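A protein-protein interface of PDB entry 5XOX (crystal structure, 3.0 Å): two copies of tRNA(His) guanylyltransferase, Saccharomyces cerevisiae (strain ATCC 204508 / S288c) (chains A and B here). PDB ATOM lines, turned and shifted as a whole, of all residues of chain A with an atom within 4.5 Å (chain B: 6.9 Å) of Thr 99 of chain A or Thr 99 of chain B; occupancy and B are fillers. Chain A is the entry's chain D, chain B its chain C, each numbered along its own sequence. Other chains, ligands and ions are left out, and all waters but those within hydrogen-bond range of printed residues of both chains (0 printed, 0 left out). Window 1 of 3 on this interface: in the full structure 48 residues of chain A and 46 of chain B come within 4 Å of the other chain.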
ATOM      1  N   ASP A  95      31.548  -5.663  -5.868  1.00  0.00           N
ATOM      2  CA  ASP A  95      31.349  -6.523  -4.718  1.00  0.00           C
ATOM      3  C   ASP A  95      32.598  -6.619  -3.907  1.00  0.00           C
ATOM      4  O   ASP A  95      32.570  -6.339  -2.708  1.00  0.00           O
ATOM      5  CB  ASP A  95      30.972  -7.923  -5.138  1.00  0.00           C
ATOM      6  CG  ASP A  95      29.948  -7.937  -6.208  1.00  0.00           C
ATOM      7  OD1 ASP A  95      28.741  -7.872  -5.873  1.00  0.00           O
ATOM      8  OD2 ASP A  95      30.382  -7.967  -7.384  1.00  0.00           O
ATOM      9  N   LYS A  96      33.697  -7.029  -4.545  1.00  0.00           N
ATOM     10  CA  LYS A  96      34.936  -7.171  -3.770  1.00  0.00           C
ATOM     11  C   LYS A  96      35.335  -5.837  -3.098  1.00  0.00           C
ATOM     12  O   LYS A  96      35.517  -5.778  -1.884  1.00  0.00           O
ATOM     13  CB  LYS A  96      36.081  -7.753  -4.614  1.00  0.00           C
ATOM     14  CG  LYS A  96      36.034  -9.326  -4.599  1.00  0.00           C
ATOM     15  CD  LYS A  96      37.311 -10.019  -5.057  1.00  0.00           C
ATOM     16  CE  LYS A  96      37.644 -11.296  -4.235  1.00  0.00           C
ATOM     17  NZ  LYS A  96      38.968 -11.932  -4.639  1.00  0.00           N
ATOM     18  N   LEU A  97      35.365  -4.760  -3.860  1.00  0.00           N
ATOM     19  CA  LEU A  97      35.658  -3.444  -3.300  1.00  0.00           C
ATOM     20  C   LEU A  97      34.822  -3.053  -2.066  1.00  0.00           C
ATOM     21  O   LEU A  97      35.362  -2.794  -0.963  1.00  0.00           O
ATOM     22  CB  LEU A  97      35.460  -2.447  -4.419  1.00  0.00           C
ATOM     23  CG  LEU A  97      36.792  -2.283  -5.141  1.00  0.00           C
ATOM     24  CD1 LEU A  97      36.613  -1.467  -6.403  1.00  0.00           C
ATOM     25  CD2 LEU A  97      37.814  -1.635  -4.189  1.00  0.00           C
ATOM     26  N   ALA A  98      33.504  -3.067  -2.258  1.00  0.00           N
ATOM     27  CA  ALA A  98      32.557  -2.668  -1.228  1.00  0.00           C
ATOM     28  C   ALA A  98      32.692  -3.583  -0.028  1.00  0.00           C
ATOM     29  O   ALA A  98      33.095  -3.159   1.052  1.00  0.00           O
ATOM     30  CB  ALA A  98      31.148  -2.705  -1.761  1.00  0.00           C
ATOM     31  N   THR A  99      32.435  -4.864  -0.243  1.00  0.00           N
ATOM     32  CA  THR A  99      32.384  -5.824   0.860  1.00  0.00           C
ATOM     33  C   THR A  99      33.704  -5.871   1.627  1.00  0.00           C
ATOM     34  O   THR A  99      33.724  -5.920   2.846  1.00  0.00           O
ATOM     35  CB  THR A  99      32.053  -7.238   0.363  1.00  0.00           C
ATOM     36  OG1 THR A  99      33.006  -7.623  -0.628  1.00  0.00           O
ATOM     37  CG2 THR A  99      30.701  -7.256  -0.262  1.00  0.00           C
ATOM     38  N   LEU A 100      34.806  -5.856   0.906  1.00  0.00           N
ATOM     39  CA  LEU A 100      36.081  -6.040   1.563  1.00  0.00           C
ATOM     40  C   LEU A 100      36.390  -4.836   2.415  1.00  0.00           C
ATOM     41  O   LEU A 100      36.738  -5.012   3.581  1.00  0.00           O
ATOM     42  CB  LEU A 100      37.180  -6.290   0.538  1.00  0.00           C
ATOM     43  CG  LEU A 100      37.135  -7.758   0.103  1.00  0.00           C
ATOM     44  CD1 LEU A 100      38.286  -8.086  -0.813  1.00  0.00           C
ATOM     45  CD2 LEU A 100      37.121  -8.709   1.305  1.00  0.00           C
ATOM     46  N   PHE A 101      36.239  -3.627   1.855  1.00  0.00           N
ATOM     47  CA  PHE A 101      36.474  -2.417   2.649  1.00  0.00           C
ATOM     48  C   PHE A 101      35.576  -2.478   3.904  1.00  0.00           C
ATOM     49  O   PHE A 101      36.066  -2.443   5.029  1.00  0.00           O
ATOM     50  CB  PHE A 101      36.180  -1.149   1.854  1.00  0.00           C
ATOM     51  CG  PHE A 101      37.300  -0.690   0.959  1.00  0.00           C
ATOM     52  CD1 PHE A 101      38.332  -1.537   0.597  1.00  0.00           C
ATOM     53  CD2 PHE A 101      37.279   0.601   0.423  1.00  0.00           C
ATOM     54  CE1 PHE A 101      39.354  -1.093  -0.267  1.00  0.00           C
ATOM     55  CE2 PHE A 101      38.283   1.048  -0.433  1.00  0.00           C
ATOM     56  CZ  PHE A 101      39.324   0.200  -0.775  1.00  0.00           C
ATOM     57  N   GLY A 102      34.268  -2.645   3.703  1.00  0.00           N
ATOM     58  CA  GLY A 102      33.345  -2.796   4.817  1.00  0.00           C
ATOM     59  C   GLY A 102      33.758  -3.809   5.891  1.00  0.00           C
ATOM     60  O   GLY A 102      33.809  -3.460   7.060  1.00  0.00           O
ATOM     61  N   SER A 103      34.065  -5.047   5.514  1.00  0.00           N
ATOM     62  CA  SER A 103      34.503  -6.055   6.486  1.00  0.00           C
ATOM     63  C   SER A 103      35.705  -5.585   7.224  1.00  0.00           C
ATOM     64  O   SER A 103      35.741  -5.687   8.426  1.00  0.00           O
ATOM     65  CB  SER A 103      34.857  -7.410   5.850  1.00  0.00           C
ATOM     66  OG  SER A 103      33.714  -8.103   5.386  1.00  0.00           O
ATOM     67  N   PHE A 130      27.992  -2.665   9.321  1.00  0.00           N
ATOM     68  CA  PHE A 130      27.990  -1.472   8.460  1.00  0.00           C
ATOM     69  C   PHE A 130      27.565  -1.779   7.009  1.00  0.00           C
ATOM     70  O   PHE A 130      27.874  -2.831   6.472  1.00  0.00           O
ATOM     71  CB  PHE A 130      29.370  -0.853   8.367  1.00  0.00           C
ATOM     72  CG  PHE A 130      29.894  -0.280   9.649  1.00  0.00           C
ATOM     73  CD1 PHE A 130      29.387  -0.645  10.852  1.00  0.00           C
ATOM     74  CD2 PHE A 130      30.886   0.673   9.638  1.00  0.00           C
ATOM     75  CE1 PHE A 130      29.888  -0.134  12.008  1.00  0.00           C
ATOM     76  CE2 PHE A 130      31.374   1.214  10.813  1.00  0.00           C
ATOM     77  CZ  PHE A 130      30.874   0.811  11.988  1.00  0.00           C
ATOM     78  N   ASP A 131      26.913  -0.833   6.353  1.00  0.00           N
ATOM     79  CA  ASP A 131      26.591  -0.920   4.924  1.00  0.00           C
ATOM     80  C   ASP A 131      27.853  -0.592   4.124  1.00  0.00           C
ATOM     81  O   ASP A 131      28.683   0.166   4.600  1.00  0.00           O
ATOM     82  CB  ASP A 131      25.452   0.075   4.618  1.00  0.00           C
ATOM     83  CG  ASP A 131      25.129   0.215   3.142  1.00  0.00           C
ATOM     84  OD1 ASP A 131      25.932  -0.223   2.301  1.00  0.00           O
ATOM     85  OD2 ASP A 131      24.045   0.764   2.827  1.00  0.00           O
ATOM     86  N   SER A 132      28.020  -1.124   2.920  1.00  0.00           N
ATOM     87  CA  SER A 132      29.066  -0.579   2.062  1.00  0.00           C
ATOM     88  C   SER A 132      28.660  -0.461   0.572  1.00  0.00           C
ATOM     89  O   SER A 132      27.856  -1.252   0.075  1.00  0.00           O
ATOM     90  CB  SER A 132      30.313  -1.415   2.206  1.00  0.00           C
ATOM     91  OG  SER A 132      31.369  -0.806   1.503  1.00  0.00           O
ATOM     92  N   VAL B  26      23.936 -15.667  -0.157  1.00  0.00           N
ATOM     93  CA  VAL B  26      24.943 -14.732   0.227  1.00  0.00           C
ATOM     94  C   VAL B  26      26.120 -15.539   0.708  1.00  0.00           C
ATOM     95  O   VAL B  26      26.036 -16.280   1.706  1.00  0.00           O
ATOM     96  CB  VAL B  26      24.441 -13.755   1.255  1.00  0.00           C
ATOM     97  CG1 VAL B  26      25.525 -12.730   1.570  1.00  0.00           C
ATOM     98  CG2 VAL B  26      23.247 -13.062   0.695  1.00  0.00           C
ATOM     99  N   ARG B  93      18.137  -5.760  -2.368  1.00  0.00           N
ATOM    100  CA  ARG B  93      19.290  -5.042  -2.875  1.00  0.00           C
ATOM    101  C   ARG B  93      20.596  -5.826  -2.738  1.00  0.00           C
ATOM    102  O   ARG B  93      21.004  -6.179  -1.629  1.00  0.00           O
ATOM    103  CB  ARG B  93      19.401  -3.721  -2.153  1.00  0.00           C
ATOM    104  CG  ARG B  93      19.489  -2.655  -3.160  1.00  0.00           C
ATOM    105  CD  ARG B  93      20.058  -1.427  -2.642  1.00  0.00           C
ATOM    106  NE  ARG B  93      19.020  -0.566  -2.121  1.00  0.00           N
ATOM    107  CZ  ARG B  93      19.278   0.692  -1.806  1.00  0.00           C
ATOM    108  NH1 ARG B  93      20.501   1.167  -2.027  1.00  0.00           N
ATOM    109  NH2 ARG B  93      18.336   1.478  -1.309  1.00  0.00           N
ATOM    110  N   LYS B  94      21.244  -6.101  -3.866  1.00  0.00           N
ATOM    111  CA  LYS B  94      22.520  -6.816  -3.866  1.00  0.00           C
ATOM    112  C   LYS B  94      23.534  -6.229  -2.908  1.00  0.00           C
ATOM    113  O   LYS B  94      24.095  -6.954  -2.077  1.00  0.00           O
ATOM    114  CB  LYS B  94      23.107  -6.812  -5.262  1.00  0.00           C
ATOM    115  CG  LYS B  94      22.369  -7.633  -6.292  1.00  0.00           C
ATOM    116  CD  LYS B  94      23.344  -8.513  -7.057  1.00  0.00           C
ATOM    117  CE  LYS B  94      24.009  -7.606  -8.121  1.00  0.00           C
ATOM    118  NZ  LYS B  94      24.999  -8.208  -9.053  1.00  0.00           N
ATOM    119  N   ASP B  95      23.763  -4.918  -3.032  1.00  0.00           N
ATOM    120  CA  ASP B  95      24.798  -4.254  -2.242  1.00  0.00           C
ATOM    121  C   ASP B  95      24.529  -4.468  -0.795  1.00  0.00           C
ATOM    122  O   ASP B  95      25.363  -4.981  -0.054  1.00  0.00           O
ATOM    123  CB  ASP B  95      24.873  -2.749  -2.503  1.00  0.00           C
ATOM    124  CG  ASP B  95      24.951  -2.404  -3.975  1.00  0.00           C
ATOM    125  OD1 ASP B  95      25.982  -2.712  -4.639  1.00  0.00           O
ATOM    126  OD2 ASP B  95      23.965  -1.798  -4.449  1.00  0.00           O
ATOM    127  N   LYS B  96      23.329  -4.076  -0.403  1.00  0.00           N
ATOM    128  CA  LYS B  96      22.948  -4.133   0.989  1.00  0.00           C
ATOM    129  C   LYS B  96      22.962  -5.592   1.516  1.00  0.00           C
ATOM    130  O   LYS B  96      23.508  -5.851   2.590  1.00  0.00           O
ATOM    131  CB  LYS B  96      21.584  -3.435   1.190  1.00  0.00           C
ATOM    132  CG  LYS B  96      21.610  -1.861   1.401  1.00  0.00           C
ATOM    133  CD  LYS B  96      20.145  -1.373   1.532  1.00  0.00           C
ATOM    134  CE  LYS B  96      19.763  -0.533   2.817  1.00  0.00           C
ATOM    135  NZ  LYS B  96      18.227  -0.396   3.059  1.00  0.00           N
ATOM    136  N   LEU B  97      22.431  -6.550   0.766  1.00  0.00           N
ATOM    137  CA  LEU B  97      22.490  -7.951   1.209  1.00  0.00           C
ATOM    138  C   LEU B  97      23.913  -8.392   1.500  1.00  0.00           C
ATOM    139  O   LEU B  97      24.259  -8.759   2.646  1.00  0.00           O
ATOM    140  CB  LEU B  97      21.855  -8.863   0.168  1.00  0.00           C
ATOM    141  CG  LEU B  97      20.372  -9.056   0.462  1.00  0.00           C
ATOM    142  CD1 LEU B  97      19.585  -9.845  -0.614  1.00  0.00           C
ATOM    143  CD2 LEU B  97      20.362  -9.798   1.779  1.00  0.00           C
ATOM    144  N   ALA B  98      24.743  -8.271   0.467  1.00  0.00           N
ATOM    145  CA  ALA B  98      26.142  -8.656   0.523  1.00  0.00           C
ATOM    146  C   ALA B  98      26.861  -7.952   1.664  1.00  0.00           C
ATOM    147  O   ALA B  98      27.292  -8.585   2.627  1.00  0.00           O
ATOM    148  CB  ALA B  98      26.808  -8.352  -0.808  1.00  0.00           C
ATOM    149  N   THR B  99      26.965  -6.637   1.563  1.00  0.00           N
ATOM    150  CA  THR B  99      27.771  -5.859   2.494  1.00  0.00           C
ATOM    151  C   THR B  99      27.326  -5.972   3.943  1.00  0.00           C
ATOM    152  O   THR B  99      28.158  -6.066   4.849  1.00  0.00           O
ATOM    153  CB  THR B  99      27.784  -4.396   2.071  1.00  0.00           C
ATOM    154  OG1 THR B  99      26.438  -3.956   1.920  1.00  0.00           O
ATOM    155  CG2 THR B  99      28.492  -4.233   0.762  1.00  0.00           C
ATOM    156  N   LEU B 100      26.017  -6.000   4.159  1.00  0.00           N
ATOM    157  CA  LEU B 100      25.497  -6.048   5.514  1.00  0.00           C
ATOM    158  C   LEU B 100      25.750  -7.375   6.171  1.00  0.00           C
ATOM    159  O   LEU B 100      26.210  -7.420   7.321  1.00  0.00           O
ATOM    160  CB  LEU B 100      24.015  -5.771   5.530  1.00  0.00           C
ATOM    161  CG  LEU B 100      23.681  -4.287   5.482  1.00  0.00           C
ATOM    162  CD1 LEU B 100      22.230  -4.145   5.840  1.00  0.00           C
ATOM    163  CD2 LEU B 100      24.575  -3.422   6.378  1.00  0.00           C
ATOM    164  N   PHE B 101      25.416  -8.454   5.458  1.00  0.00           N
ATOM    165  CA  PHE B 101      25.766  -9.789   5.956  1.00  0.00           C
ATOM    166  C   PHE B 101      27.261  -9.937   6.247  1.00  0.00           C
ATOM    167  O   PHE B 101      27.669 -10.558   7.245  1.00  0.00           O
ATOM    168  CB  PHE B 101      25.314 -10.875   4.975  1.00  0.00           C
ATOM    169  CG  PHE B 101      23.851 -11.206   5.067  1.00  0.00           C
ATOM    170  CD1 PHE B 101      22.989 -10.433   5.840  1.00  0.00           C
ATOM    171  CD2 PHE B 101      23.341 -12.311   4.409  1.00  0.00           C
ATOM    172  CE1 PHE B 101      21.634 -10.747   5.946  1.00  0.00           C
ATOM    173  CE2 PHE B 101      21.989 -12.628   4.503  1.00  0.00           C
ATOM    174  CZ  PHE B 101      21.130 -11.839   5.278  1.00  0.00           C
ATOM    175  N   GLY B 102      28.068  -9.363   5.367  1.00  0.00           N
ATOM    176  CA  GLY B 102      29.498  -9.390   5.554  1.00  0.00           C
ATOM    177  C   GLY B 102      29.898  -8.704   6.844  1.00  0.00           C
ATOM    178  O   GLY B 102      30.573  -9.320   7.688  1.00  0.00           O
ATOM    179  N   SER B 103      29.497  -7.442   7.005  1.00  0.00           N
ATOM    180  CA  SER B 103      29.867  -6.710   8.220  1.00  0.00           C
ATOM    181  C   SER B 103      29.504  -7.558   9.406  1.00  0.00           C
ATOM    182  O   SER B 103      30.351  -7.864  10.224  1.00  0.00           O
ATOM    183  CB  SER B 103      29.183  -5.343   8.343  1.00  0.00           C
ATOM    184  OG  SER B 103      29.751  -4.391   7.469  1.00  0.00           O
ATOM    185  N   PHE B 104      28.250  -7.993   9.432  1.00  0.00           N
ATOM    186  CA  PHE B 104      27.693  -8.641  10.601  1.00  0.00           C
ATOM    187  C   PHE B 104      28.546  -9.835  11.004  1.00  0.00           C
ATOM    188  O   PHE B 104      29.008  -9.937  12.139  1.00  0.00           O
ATOM    189  CB  PHE B 104      26.289  -9.123  10.321  1.00  0.00           C
ATOM    190  CG  PHE B 104      25.596  -9.652  11.530  1.00  0.00           C
ATOM    191  CD1 PHE B 104      25.503  -8.856  12.665  1.00  0.00           C
ATOM    192  CD2 PHE B 104      25.072 -10.932  11.566  1.00  0.00           C
ATOM    193  CE1 PHE B 104      24.873  -9.292  13.786  1.00  0.00           C
ATOM    194  CE2 PHE B 104      24.436 -11.384  12.706  1.00  0.00           C
ATOM    195  CZ  PHE B 104      24.340 -10.555  13.817  1.00  0.00           C
ATOM    196  N   THR B 106      31.651 -10.738  10.084  1.00  0.00           N
ATOM    197  CA  THR B 106      32.915 -10.217  10.549  1.00  0.00           C
ATOM    198  C   THR B 106      32.858  -9.719  11.987  1.00  0.00           C
ATOM    199  O   THR B 106      33.611 -10.185  12.841  1.00  0.00           O
ATOM    200  CB  THR B 106      33.389  -9.081   9.632  1.00  0.00           C
ATOM    201  OG1 THR B 106      33.953  -9.618   8.412  1.00  0.00           O
ATOM    202  CG2 THR B 106      34.360  -8.176  10.354  1.00  0.00           C
ATOM    203  N   TYR B 129      39.182 -10.436   7.973  1.00  0.00           N
ATOM    204  CA  TYR B 129      38.147  -9.760   7.206  1.00  0.00           C
ATOM    205  C   TYR B 129      37.740 -10.619   6.013  1.00  0.00           C
ATOM    206  O   TYR B 129      38.539 -11.415   5.497  1.00  0.00           O
ATOM    207  CB  TYR B 129      38.616  -8.374   6.790  1.00  0.00           C
ATOM    208  CG  TYR B 129      39.757  -8.348   5.827  1.00  0.00           C
ATOM    209  CD1 TYR B 129      40.990  -8.831   6.179  1.00  0.00           C
ATOM    210  CD2 TYR B 129      39.620  -7.761   4.592  1.00  0.00           C
ATOM    211  CE1 TYR B 129      42.059  -8.766   5.297  1.00  0.00           C
ATOM    212  CE2 TYR B 129      40.675  -7.689   3.706  1.00  0.00           C
ATOM    213  CZ  TYR B 129      41.896  -8.187   4.061  1.00  0.00           C
ATOM    214  OH  TYR B 129      42.957  -8.119   3.178  1.00  0.00           O
ATOM    215  N   PHE B 130      36.462 -10.515   5.647  1.00  0.00           N
ATOM    216  CA  PHE B 130      35.855 -11.452   4.707  1.00  0.00           C
ATOM    217  C   PHE B 130      35.226 -10.759   3.468  1.00  0.00           C
ATOM    218  O   PHE B 130      34.709  -9.643   3.558  1.00  0.00           O
ATOM    219  CB  PHE B 130      34.770 -12.278   5.416  1.00  0.00           C
ATOM    220  CG  PHE B 130      35.252 -13.145   6.571  1.00  0.00           C
ATOM    221  CD1 PHE B 130      36.536 -13.122   7.028  1.00  0.00           C
ATOM    222  CD2 PHE B 130      34.371 -13.978   7.219  1.00  0.00           C
ATOM    223  CE1 PHE B 130      36.933 -13.926   8.096  1.00  0.00           C
ATOM    224  CE2 PHE B 130      34.769 -14.782   8.284  1.00  0.00           C
ATOM    225  CZ  PHE B 130      36.049 -14.758   8.716  1.00  0.00           C
ATOM    226  N   ASP B 131      35.286 -11.448   2.324  1.00  0.00           N
ATOM    227  CA  ASP B 131      34.595 -11.118   1.066  1.00  0.00           C
ATOM    228  C   ASP B 131      33.110 -11.543   1.112  1.00  0.00           C
ATOM    229  O   ASP B 131      32.773 -12.554   1.755  1.00  0.00           O
ATOM    230  CB  ASP B 131      35.297 -11.837  -0.091  1.00  0.00           C
ATOM    231  CG  ASP B 131      34.514 -11.796  -1.385  1.00  0.00           C
ATOM    232  OD1 ASP B 131      33.393 -11.257  -1.411  1.00  0.00           O
ATOM    233  OD2 ASP B 131      35.056 -12.244  -2.411  1.00  0.00           O
ATOM    234  N   SER B 132      32.238 -10.817   0.399  1.00  0.00           N
ATOM    235  CA  SER B 132      30.827 -11.209   0.275  1.00  0.00           C
ATOM    236  C   SER B 132      30.174 -11.026  -1.108  1.00  0.00           C
ATOM    237  O   SER B 132      30.469 -10.068  -1.831  1.00  0.00           O
ATOM    238  CB  SER B 132      30.001 -10.448   1.284  1.00  0.00           C
ATOM    239  OG  SER B 132      28.629 -10.694   1.051  1.00  0.00           O
ATOM    240  N   ARG B 133      29.268 -11.951  -1.461  1.00  0.00           N
ATOM    241  CA  ARG B 133      28.610 -11.965  -2.785  1.00  0.00           C
ATOM    242  C   ARG B 133      27.143 -12.257  -2.627  1.00  0.00           C
ATOM    243  O   ARG B 133      26.769 -12.996  -1.720  1.00  0.00           O
ATOM    244  CB  ARG B 133      29.160 -13.063  -3.704  1.00  0.00           C
ATOM    245  CG  ARG B 133      30.586 -13.225  -3.545  1.00  0.00           C
ATOM    246  CD  ARG B 133      30.999 -14.621  -3.842  1.00  0.00           C
ATOM    247  NE  ARG B 133      32.390 -14.543  -4.219  1.00  0.00           N
ATOM    248  CZ  ARG B 133      32.784 -14.267  -5.434  1.00  0.00           C
ATOM    249  NH1 ARG B 133      31.885 -14.063  -6.381  1.00  0.00           N
ATOM    250  NH2 ARG B 133      34.069 -14.192  -5.680  1.00  0.00           N
ATOM    251  N   CYS B 134      26.330 -11.756  -3.557  1.00  0.00           N
ATOM    252  CA  CYS B 134      24.972 -12.273  -3.773  1.00  0.00           C
ATOM    253  C   CYS B 134      24.809 -13.112  -5.047  1.00  0.00           C
ATOM    254  O   CYS B 134      25.278 -12.735  -6.124  1.00  0.00           O
ATOM    255  CB  CYS B 134      23.994 -11.121  -3.842  1.00  0.00           C
ATOM    256  SG  CYS B 134      23.542 -10.627  -2.232  1.00  0.00           S
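Asp 95 of chain A touches Ser 132 of chain B, but with the chains exchanged Ser 132 of chain A does not touch Asp 95 of chain B (4.2 Å).
Thr 99 of chain A touches Phe 130 of chain B, and with the chains exchanged Phe 130 of chain A touches Thr 99 of chain B.
Thr 99 of chain A touches Asp 131 of chain B, and with the chains exchanged Asp 131 of chain A touches Thr 99 of chain B.
Thr 99 of chain A touches Ser 132 of chain B, and with the chains exchanged Ser 132 of chain A touches Thr 99 of chain B.
12 positions are printed for both chains.
Of the 19 pairs that touch across the chains among the printed residues, 15 have their exchanged pair printed and touching as well.
N of Ser 132 of chain A sits close to OG1 of Thr 99 of chain B.
The side-chain hydroxyl of Ser 103 of chain B sits at hydrogen-bond distance from the backbone carbonyl oxygen of Phe 130 of chain A (2.6 Å).
The side-chain hydroxyl of Thr 106 of chain B sits at hydrogen-bond distance from the side-chain hydroxyl of Ser 103 of chain A, at 3.4 Å.
The backbone carbonyl oxygen (O) of Phe 130 of chain B sits at hydrogen-bond distance from the side-chain hydroxyl (OG) of Ser 103 of chain A (2.6 Å).
The side-chain hydroxyl (OG1) of Thr 99 of chain A sits at hydrogen-bond distance from the backbone NH (N) of Ser 132 of chain B.
The side-chain hydroxyl of Thr 99 of chain B is in hydrogen-bond range of the backbone carbonyl oxygen of Asp 95 of chain B (2.5 Å).
The side-chain hydroxyl (OG) of Ser 103 of chain B lies within hydrogen-bond range of the backbone carbonyl oxygen (O) of Thr 99 of chain B (3.5 Å).
The backbone carbonyl oxygen (O) of Gly 102 of chain B lies close to the side-chain hydroxyl (OG1) of Thr 106 of chain B (3.5 Å).
The side-chain hydroxyl of Thr 99 of chain A is in hydrogen-bond range of the backbone carbonyl oxygen of Asp 95 of chain A (2.5 Å).
The backbone carbonyl oxygen of Ala 98 of chain A lies within hydrogen-bond range of the side-chain hydroxyl of Ser 132 of chain A (3.0 Å).
The side-chain hydroxyl (OG) of Ser 103 of chain A is in hydrogen-bond range of the backbone carbonyl oxygen (O) of Thr 99 of chain A (3.3 Å).
Of the 20 printed residues of chain B, 9 touch a printed residue of chain A.
Hydrophobic or aromatic side chains of chain B within 4 Å of the printed part of chain A: Leu 100 and Tyr 129.
Hydrophobic or aromatic side chains of chain A that line the printed part of chain B: Ala 98, Leu 100 and Phe 130.
Among the printed residues, no Asp or Glu carboxylate lies within 4 Å of a Lys or Arg side-chain nitrogen of the other chain.
Thr 99 of chain B touches five residues of chain A.
Printed residues of chain A within 4 Å of Ser 132 of chain B: Asp 95 (3.97 Å) and Thr 99 (3.2 Å).
Of the printed residues of chain A, Lys 96 of chain B touches Asp 131 (3.9 Å).
Printed residues of chain A within 4 Å of Phe 130 of chain B: Thr 99, Leu 100 and Ser 103.
Printed residues of chain B within 4 Å of Ser 103 of chain A: Thr 106, Tyr 129 and Phe 130.
Of the printed residues of chain A, Ser 103 of chain B touches Phe 130.
Asp 95 of chain B touches none of the printed residues of chain A.
Arg 93 of chain B touches none of the printed residues of chain A.
The nearest printed residue of chain B that does not touch Asp 131 of chain A is Ser 103 of chain B (4.7 Å).
Among the printed residues, merely in contact across the chains: Lys 96 of chain A with Asp 131 of chain B, Phe 130 of chain A with Leu 100 of chain B, Leu 100 of chain A with Phe 130 of chain B, Leu 100 of chain A with Asp 131 of chain B, Asp 131 of chain A with Leu 100 of chain B, Phe 130 of chain A with Thr 99 of chain B, Thr 99 of chain A with Asp 131 of chain B, Asp 131 of chain A with Thr 99 of chain B, Asp 131 of chain A with Lys 96 of chain B, Thr 99 of chain A with Thr 99 of chain B, Thr 99 of chain A with Phe 130 of chain B, Ala 98 of chain A with Thr 99 of chain B, Asp 95 of chain A with Ser 132 of chain B and Ser 103 of chain A with Tyr 129 of chain B.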
